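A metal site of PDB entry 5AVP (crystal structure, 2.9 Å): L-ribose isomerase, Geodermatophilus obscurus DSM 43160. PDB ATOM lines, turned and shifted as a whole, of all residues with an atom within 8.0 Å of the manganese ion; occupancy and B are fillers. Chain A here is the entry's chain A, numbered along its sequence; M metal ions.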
ATOM      1  N   MET A  83      16.144  -7.776 -26.404  1.00  0.00           N
ATOM      2  CA  MET A  83      16.267  -9.159 -25.943  1.00  0.00           C
ATOM      3  C   MET A  83      15.473 -10.138 -26.801  1.00  0.00           C
ATOM      4  O   MET A  83      14.653  -9.742 -27.627  1.00  0.00           O
ATOM      5  CB  MET A  83      15.802  -9.294 -24.486  1.00  0.00           C
ATOM      6  CG  MET A  83      14.288  -9.152 -24.336  1.00  0.00           C
ATOM      7  SD  MET A  83      13.695  -9.173 -22.668  1.00  0.00           S
ATOM      8  CE  MET A  83      14.130 -10.801 -22.182  1.00  0.00           C
ATOM      9  N   ILE A  85      13.103 -13.750 -26.553  1.00  0.00           N
ATOM     10  CA  ILE A  85      12.348 -14.565 -25.611  1.00  0.00           C
ATOM     11  C   ILE A  85      11.714 -15.772 -26.290  1.00  0.00           C
ATOM     12  O   ILE A  85      10.795 -15.612 -27.092  1.00  0.00           O
ATOM     13  CB  ILE A  85      11.236 -13.725 -24.935  1.00  0.00           C
ATOM     14  CG1 ILE A  85      11.826 -12.469 -24.331  1.00  0.00           C
ATOM     15  CG2 ILE A  85      10.544 -14.524 -23.835  1.00  0.00           C
ATOM     16  CD1 ILE A  85      10.796 -11.552 -23.724  1.00  0.00           C
ATOM     17  N   LYS A 113       9.628 -19.548 -20.211  1.00  0.00           N
ATOM     18  CA  LYS A 113      10.381 -19.002 -21.321  1.00  0.00           C
ATOM     19  C   LYS A 113      11.835 -18.741 -20.959  1.00  0.00           C
ATOM     20  O   LYS A 113      12.178 -18.485 -19.808  1.00  0.00           O
ATOM     21  CB  LYS A 113       9.740 -17.703 -21.793  1.00  0.00           C
ATOM     22  CG  LYS A 113       9.671 -16.633 -20.738  1.00  0.00           C
ATOM     23  CD  LYS A 113       8.896 -15.447 -21.248  1.00  0.00           C
ATOM     24  CE  LYS A 113       7.514 -15.868 -21.687  1.00  0.00           C
ATOM     25  NZ  LYS A 113       6.613 -14.702 -21.653  1.00  0.00           N
ATOM     26  N   MET A 115      15.179 -16.402 -21.763  1.00  0.00           N
ATOM     27  CA  MET A 115      15.436 -15.055 -22.259  1.00  0.00           C
ATOM     28  C   MET A 115      16.935 -14.847 -22.463  1.00  0.00           C
ATOM     29  O   MET A 115      17.755 -15.296 -21.643  1.00  0.00           O
ATOM     30  CB  MET A 115      14.851 -14.027 -21.283  1.00  0.00           C
ATOM     31  CG  MET A 115      13.439 -14.383 -20.815  1.00  0.00           C
ATOM     32  SD  MET A 115      12.664 -13.199 -19.682  1.00  0.00           S
ATOM     33  CE  MET A 115      13.811 -13.227 -18.296  1.00  0.00           C
ATOM     34  N   CYS A 123      16.375  -5.104 -20.142  1.00  0.00           N
ATOM     35  CA  CYS A 123      14.979  -5.511 -20.289  1.00  0.00           C
ATOM     36  C   CYS A 123      14.390  -4.342 -19.496  1.00  0.00           C
ATOM     37  O   CYS A 123      14.386  -4.370 -18.272  1.00  0.00           O
ATOM     38  CB  CYS A 123      14.680  -6.830 -19.567  1.00  0.00           C
ATOM     39  SG  CYS A 123      12.862  -7.131 -19.311  1.00  0.00           S
ATOM     40  N   PRO A 124      13.902  -3.318 -20.200  1.00  0.00           N
ATOM     41  CA  PRO A 124      13.302  -2.073 -19.698  1.00  0.00           C
ATOM     42  C   PRO A 124      12.413  -2.115 -18.448  1.00  0.00           C
ATOM     43  O   PRO A 124      11.690  -3.099 -18.239  1.00  0.00           O
ATOM     44  CB  PRO A 124      12.518  -1.575 -20.902  1.00  0.00           C
ATOM     45  CG  PRO A 124      12.084  -2.845 -21.526  1.00  0.00           C
ATOM     46  CD  PRO A 124      13.404  -3.581 -21.550  1.00  0.00           C
ATOM     47  N   HIS A 126       9.493  -2.081 -16.086  1.00  0.00           N
ATOM     48  CA  HIS A 126       8.085  -2.373 -16.291  1.00  0.00           C
ATOM     49  C   HIS A 126       7.557  -3.158 -15.094  1.00  0.00           C
ATOM     50  O   HIS A 126       8.329  -3.691 -14.292  1.00  0.00           O
ATOM     51  CB  HIS A 126       7.871  -3.215 -17.547  1.00  0.00           C
ATOM     52  CG  HIS A 126       8.301  -4.648 -17.394  1.00  0.00           C
ATOM     53  ND1 HIS A 126       9.612  -5.072 -17.571  1.00  0.00           N
ATOM     54  CD2 HIS A 126       7.603  -5.753 -17.026  1.00  0.00           C
ATOM     55  CE1 HIS A 126       9.691  -6.365 -17.321  1.00  0.00           C
ATOM     56  NE2 HIS A 126       8.495  -6.800 -16.983  1.00  0.00           N
ATOM     57  N   TYR A 127       6.237  -3.218 -14.981  1.00  0.00           N
ATOM     58  CA  TYR A 127       5.579  -3.974 -13.925  1.00  0.00           C
ATOM     59  C   TYR A 127       4.350  -4.625 -14.544  1.00  0.00           C
ATOM     60  O   TYR A 127       3.832  -4.154 -15.545  1.00  0.00           O
ATOM     61  CB  TYR A 127       5.168  -3.071 -12.748  1.00  0.00           C
ATOM     62  CG  TYR A 127       3.958  -2.186 -12.972  1.00  0.00           C
ATOM     63  CD1 TYR A 127       2.679  -2.714 -13.017  1.00  0.00           C
ATOM     64  CD2 TYR A 127       4.109  -0.806 -13.142  1.00  0.00           C
ATOM     65  CE1 TYR A 127       1.579  -1.908 -13.234  1.00  0.00           C
ATOM     66  CE2 TYR A 127       3.013   0.013 -13.361  1.00  0.00           C
ATOM     67  CZ  TYR A 127       1.752  -0.551 -13.413  1.00  0.00           C
ATOM     68  OH  TYR A 127       0.655   0.247 -13.676  1.00  0.00           O
ATOM     69  N   HIS A 128       3.914  -5.723 -13.956  1.00  0.00           N
ATOM     70  CA  HIS A 128       2.747  -6.439 -14.462  1.00  0.00           C
ATOM     71  C   HIS A 128       1.713  -6.412 -13.371  1.00  0.00           C
ATOM     72  O   HIS A 128       2.036  -6.496 -12.184  1.00  0.00           O
ATOM     73  CB  HIS A 128       3.091  -7.892 -14.775  1.00  0.00           C
ATOM     74  CG  HIS A 128       4.376  -8.064 -15.526  1.00  0.00           C
ATOM     75  ND1 HIS A 128       4.446  -7.994 -16.889  1.00  0.00           N
ATOM     76  CD2 HIS A 128       5.637  -8.285 -15.085  1.00  0.00           C
ATOM     77  CE1 HIS A 128       5.702  -8.175 -17.275  1.00  0.00           C
ATOM     78  NE2 HIS A 128       6.438  -8.351 -16.187  1.00  0.00           N
ATOM     79  N   LYS A 131       0.813 -10.815 -13.639  1.00  0.00           N
ATOM     80  CA  LYS A 131       1.948 -11.724 -13.658  1.00  0.00           C
ATOM     81  C   LYS A 131       2.959 -11.623 -12.526  1.00  0.00           C
ATOM     82  O   LYS A 131       3.379 -10.542 -12.120  1.00  0.00           O
ATOM     83  CB  LYS A 131       2.680 -11.608 -15.010  1.00  0.00           C
ATOM     84  CG  LYS A 131       3.671 -12.711 -15.259  1.00  0.00           C
ATOM     85  CD  LYS A 131       4.282 -12.644 -16.648  1.00  0.00           C
ATOM     86  CE  LYS A 131       5.414 -11.636 -16.776  1.00  0.00           C
ATOM     87  NZ  LYS A 131       6.454 -12.118 -17.733  1.00  0.00           N
ATOM     88  N   THR A 132       3.336 -12.795 -12.012  1.00  0.00           N
ATOM     89  CA  THR A 132       4.365 -12.914 -10.980  1.00  0.00           C
ATOM     90  C   THR A 132       5.412 -13.819 -11.616  1.00  0.00           C
ATOM     91  O   THR A 132       5.095 -14.903 -12.136  1.00  0.00           O
ATOM     92  CB  THR A 132       3.866 -13.585  -9.698  1.00  0.00           C
ATOM     93  OG1 THR A 132       3.191 -12.610  -8.884  1.00  0.00           O
ATOM     94  CG2 THR A 132       5.035 -14.136  -8.930  1.00  0.00           C
ATOM     95  N   GLU A 133       6.651 -13.361 -11.578  1.00  0.00           N
ATOM     96  CA  GLU A 133       7.763 -14.068 -12.203  1.00  0.00           C
ATOM     97  C   GLU A 133       8.800 -14.649 -11.242  1.00  0.00           C
ATOM     98  O   GLU A 133       8.927 -14.219 -10.090  1.00  0.00           O
ATOM     99  CB  GLU A 133       8.479 -13.117 -13.171  1.00  0.00           C
ATOM    100  CG  GLU A 133       7.583 -12.131 -13.905  1.00  0.00           C
ATOM    101  CD  GLU A 133       8.365 -11.135 -14.770  1.00  0.00           C
ATOM    102  OE1 GLU A 133       9.482 -10.742 -14.384  1.00  0.00           O
ATOM    103  OE2 GLU A 133       7.846 -10.708 -15.822  1.00  0.00           O
ATOM    104  N   TYR A 135      13.037 -16.131 -11.435  1.00  0.00           N
ATOM    105  CA  TYR A 135      14.226 -16.139 -12.305  1.00  0.00           C
ATOM    106  C   TYR A 135      15.210 -17.249 -11.948  1.00  0.00           C
ATOM    107  O   TYR A 135      15.458 -17.537 -10.791  1.00  0.00           O
ATOM    108  CB  TYR A 135      14.963 -14.798 -12.217  1.00  0.00           C
ATOM    109  CG  TYR A 135      14.103 -13.576 -12.440  1.00  0.00           C
ATOM    110  CD1 TYR A 135      13.548 -13.292 -13.695  1.00  0.00           C
ATOM    111  CD2 TYR A 135      13.817 -12.693 -11.392  1.00  0.00           C
ATOM    112  CE1 TYR A 135      12.748 -12.175 -13.894  1.00  0.00           C
ATOM    113  CE2 TYR A 135      13.027 -11.592 -11.579  1.00  0.00           C
ATOM    114  CZ  TYR A 135      12.490 -11.328 -12.825  1.00  0.00           C
ATOM    115  OH  TYR A 135      11.687 -10.215 -13.000  1.00  0.00           O
ATOM    116  N   MET A 202       9.594 -12.427  -8.265  1.00  0.00           N
ATOM    117  CA  MET A 202       9.241 -11.024  -8.513  1.00  0.00           C
ATOM    118  C   MET A 202       7.734 -10.905  -8.568  1.00  0.00           C
ATOM    119  O   MET A 202       7.127 -11.203  -9.597  1.00  0.00           O
ATOM    120  CB  MET A 202       9.831 -10.530  -9.834  1.00  0.00           C
ATOM    121  CG  MET A 202       9.506  -9.064 -10.161  1.00  0.00           C
ATOM    122  SD  MET A 202      10.056  -7.854  -8.878  1.00  0.00           S
ATOM    123  CE  MET A 202      11.846  -8.061  -8.979  1.00  0.00           C
ATOM    124  N   HIS A 206       5.161  -5.069  -9.113  1.00  0.00           N
ATOM    125  CA  HIS A 206       6.473  -4.553  -8.748  1.00  0.00           C
ATOM    126  C   HIS A 206       7.268  -4.135  -9.985  1.00  0.00           C
ATOM    127  O   HIS A 206       7.326  -4.876 -10.966  1.00  0.00           O
ATOM    128  CB  HIS A 206       7.251  -5.600  -7.970  1.00  0.00           C
ATOM    129  CG  HIS A 206       6.807  -5.725  -6.559  1.00  0.00           C
ATOM    130  ND1 HIS A 206       7.118  -4.788  -5.597  1.00  0.00           N
ATOM    131  CD2 HIS A 206       6.048  -6.664  -5.937  1.00  0.00           C
ATOM    132  CE1 HIS A 206       6.574  -5.148  -4.439  1.00  0.00           C
ATOM    133  NE2 HIS A 206       5.920  -6.282  -4.629  1.00  0.00           N
ATOM    134  N   HIS A 208      10.242  -3.857 -12.237  1.00  0.00           N
ATOM    135  CA  HIS A 208      11.500  -4.558 -12.374  1.00  0.00           C
ATOM    136  C   HIS A 208      12.168  -4.293 -13.712  1.00  0.00           C
ATOM    137  O   HIS A 208      11.594  -3.655 -14.604  1.00  0.00           O
ATOM    138  CB  HIS A 208      11.339  -6.078 -12.152  1.00  0.00           C
ATOM    139  CG  HIS A 208      10.482  -6.776 -13.187  1.00  0.00           C
ATOM    140  ND1 HIS A 208       9.102  -6.807 -13.113  1.00  0.00           N
ATOM    141  CD2 HIS A 208      10.819  -7.528 -14.256  1.00  0.00           C
ATOM    142  CE1 HIS A 208       8.636  -7.562 -14.096  1.00  0.00           C
ATOM    143  NE2 HIS A 208       9.657  -8.011 -14.798  1.00  0.00           N
ATOM    144  N   ALA A 209      13.406  -4.774 -13.815  1.00  0.00           N
ATOM    145  CA  ALA A 209      14.224  -4.612 -15.010  1.00  0.00           C
ATOM    146  C   ALA A 209      15.590  -5.209 -14.676  1.00  0.00           C
ATOM    147  O   ALA A 209      16.093  -5.018 -13.576  1.00  0.00           O
ATOM    148  CB  ALA A 209      14.372  -3.120 -15.363  1.00  0.00           C
ATOM    149  N   PHE A 210      16.172  -5.933 -15.625  1.00  0.00           N
ATOM    150  CA  PHE A 210      17.471  -6.544 -15.432  1.00  0.00           C
ATOM    151  C   PHE A 210      18.358  -6.300 -16.640  1.00  0.00           C
ATOM    152  O   PHE A 210      17.893  -5.883 -17.689  1.00  0.00           O
ATOM    153  CB  PHE A 210      17.313  -8.037 -15.227  1.00  0.00           C
ATOM    154  CG  PHE A 210      16.574  -8.714 -16.329  1.00  0.00           C
ATOM    155  CD1 PHE A 210      17.157  -8.889 -17.582  1.00  0.00           C
ATOM    156  CD2 PHE A 210      15.276  -9.172 -16.126  1.00  0.00           C
ATOM    157  CE1 PHE A 210      16.464  -9.504 -18.619  1.00  0.00           C
ATOM    158  CE2 PHE A 210      14.569  -9.798 -17.159  1.00  0.00           C
ATOM    159  CZ  PHE A 210      15.162  -9.966 -18.393  1.00  0.00           C
ATOM    160  N   GLU A 224      12.635 -18.076 -17.202  1.00  0.00           N
ATOM    161  CA  GLU A 224      11.598 -17.374 -16.491  1.00  0.00           C
ATOM    162  C   GLU A 224      10.375 -18.265 -16.324  1.00  0.00           C
ATOM    163  O   GLU A 224       9.744 -18.646 -17.305  1.00  0.00           O
ATOM    164  CB  GLU A 224      11.190 -16.112 -17.244  1.00  0.00           C
ATOM    165  CG  GLU A 224      10.152 -15.263 -16.498  1.00  0.00           C
ATOM    166  CD  GLU A 224       9.384 -14.345 -17.429  1.00  0.00           C
ATOM    167  OE1 GLU A 224      10.036 -13.511 -18.085  1.00  0.00           O
ATOM    168  OE2 GLU A 224       8.148 -14.463 -17.490  1.00  0.00           O
ATOM    169  N   SER A 226       6.832 -18.103 -14.751  1.00  0.00           N
ATOM    170  CA  SER A 226       5.901 -17.109 -14.228  1.00  0.00           C
ATOM    171  C   SER A 226       4.454 -17.501 -14.439  1.00  0.00           C
ATOM    172  O   SER A 226       4.159 -18.565 -14.983  1.00  0.00           O
ATOM    173  CB  SER A 226       6.137 -15.812 -14.979  1.00  0.00           C
ATOM    174  OG  SER A 226       5.713 -15.958 -16.336  1.00  0.00           O
ATOM    175  N   SER A 229       1.219 -15.216 -19.352  1.00  0.00           N
ATOM    176  CA  SER A 229       1.712 -14.025 -20.061  1.00  0.00           C
ATOM    177  C   SER A 229       0.671 -13.504 -21.035  1.00  0.00           C
ATOM    178  O   SER A 229       0.452 -14.100 -22.089  1.00  0.00           O
ATOM    179  CB  SER A 229       2.970 -14.361 -20.875  1.00  0.00           C
ATOM    180  OG  SER A 229       4.153 -14.289 -20.108  1.00  0.00           O
ATOM    181  N   ASP A 251      -0.934  -6.808 -19.970  1.00  0.00           N
ATOM    182  CA  ASP A 251      -0.359  -7.067 -18.655  1.00  0.00           C
ATOM    183  C   ASP A 251       1.071  -6.536 -18.508  1.00  0.00           C
ATOM    184  O   ASP A 251       1.711  -6.698 -17.482  1.00  0.00           O
ATOM    185  CB  ASP A 251      -0.402  -8.588 -18.386  1.00  0.00           C
ATOM    186  CG  ASP A 251      -0.533  -8.924 -16.922  1.00  0.00           C
ATOM    187  OD1 ASP A 251      -1.350  -8.280 -16.231  1.00  0.00           O
ATOM    188  OD2 ASP A 251       0.170  -9.856 -16.464  1.00  0.00           O
ATOM    189  N   ASN A 252       1.560  -5.899 -19.567  1.00  0.00           N
ATOM    190  CA  ASN A 252       2.891  -5.328 -19.580  1.00  0.00           C
ATOM    191  C   ASN A 252       2.793  -3.821 -19.509  1.00  0.00           C
ATOM    192  O   ASN A 252       2.249  -3.203 -20.420  1.00  0.00           O
ATOM    193  CB  ASN A 252       3.614  -5.678 -20.859  1.00  0.00           C
ATOM    194  CG  ASN A 252       3.643  -7.141 -21.101  1.00  0.00           C
ATOM    195  OD1 ASN A 252       4.403  -7.856 -20.457  1.00  0.00           O
ATOM    196  ND2 ASN A 252       2.799  -7.604 -22.024  1.00  0.00           N
ATOM    197  N   PHE A 254       5.247  -0.664 -19.161  1.00  0.00           N
ATOM    198  CA  PHE A 254       6.595  -0.112 -19.165  1.00  0.00           C
ATOM    199  C   PHE A 254       6.644   1.357 -18.749  1.00  0.00           C
ATOM    200  O   PHE A 254       5.831   2.168 -19.201  1.00  0.00           O
ATOM    201  CB  PHE A 254       7.195  -0.215 -20.569  1.00  0.00           C
ATOM    202  CG  PHE A 254       7.217  -1.605 -21.119  1.00  0.00           C
ATOM    203  CD1 PHE A 254       6.046  -2.349 -21.238  1.00  0.00           C
ATOM    204  CD2 PHE A 254       8.413  -2.158 -21.574  1.00  0.00           C
ATOM    205  CE1 PHE A 254       6.053  -3.623 -21.791  1.00  0.00           C
ATOM    206  CE2 PHE A 254       8.429  -3.419 -22.116  1.00  0.00           C
ATOM    207  CZ  PHE A 254       7.240  -4.156 -22.229  1.00  0.00           C
ATOM    208  N   ARG A 263       7.660  -3.236 -27.724  1.00  0.00           N
ATOM    209  CA  ARG A 263       7.454  -4.627 -27.322  1.00  0.00           C
ATOM    210  C   ARG A 263       6.444  -5.299 -28.248  1.00  0.00           C
ATOM    211  O   ARG A 263       6.542  -6.504 -28.467  1.00  0.00           O
ATOM    212  CB  ARG A 263       6.980  -4.752 -25.870  1.00  0.00           C
ATOM    213  CG  ARG A 263       6.682  -6.184 -25.433  1.00  0.00           C
ATOM    214  CD  ARG A 263       7.848  -6.873 -24.691  1.00  0.00           C
ATOM    215  NE  ARG A 263       7.717  -6.819 -23.218  1.00  0.00           N
ATOM    216  CZ  ARG A 263       8.240  -7.708 -22.370  1.00  0.00           C
ATOM    217  NH1 ARG A 263       8.936  -8.732 -22.829  1.00  0.00           N
ATOM    218  NH2 ARG A 263       8.062  -7.564 -21.055  1.00  0.00           N
HETATM  219 MN    MN M   1       8.650  -9.008 -16.685  1.00  0.00          MN
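The side-chain amino group (NZ) of Lys 131 sits close to the side-chain carboxylate (OE2) of Glu 133 (2.8 Å). The side-chain carboxylate of Glu 133 sits at hydrogen-bond distance from the side-chain hydroxyl of Tyr 135 (2.7 Å). The backbone carbonyl oxygen (O) of Glu 133 sits at hydrogen-bond distance from the backbone NH (N) of Met 202, 2.6 Å away. The backbone carbonyl oxygen (O) of Pro 124 is in hydrogen-bond range of a ring nitrogen (ND1) of His 126, at 2.9 Å. The side-chain hydroxyl (OH) of Tyr 135 sits close to a ring nitrogen (NE2) of His 208 (3.5 Å). The backbone carbonyl oxygen of Asp 251 is in hydrogen-bond range of a ring nitrogen (ND1) of His 128 (3.1 Å). OE2 of Glu 224 is in salt-bridge range of NZ of Lys 131 (2.9 Å). The backbone NH (N) of Lys 131 lies within hydrogen-bond range of the side-chain carboxylate (OD2) of Asp 251 (3.1 Å).
Lys 131 touches the manganese ion. Of the 25 residues printed, 5 come within 4 Å of the manganese ion. Along chain A the residues within 4 Å of the manganese ion span positions 126 to 208. The nearest printed residue that does not touch the manganese ion is Arg 263 (4.6 Å).
The manganese ion is bound by OE2 of Glu 133 (2.1 Å), NE2 of His 126 (2.2 Å), NE2 of His 208 (2.4 Å) and NE2 of His 128 (2.4 Å). The manganese ion has four donor atoms within binding distance.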
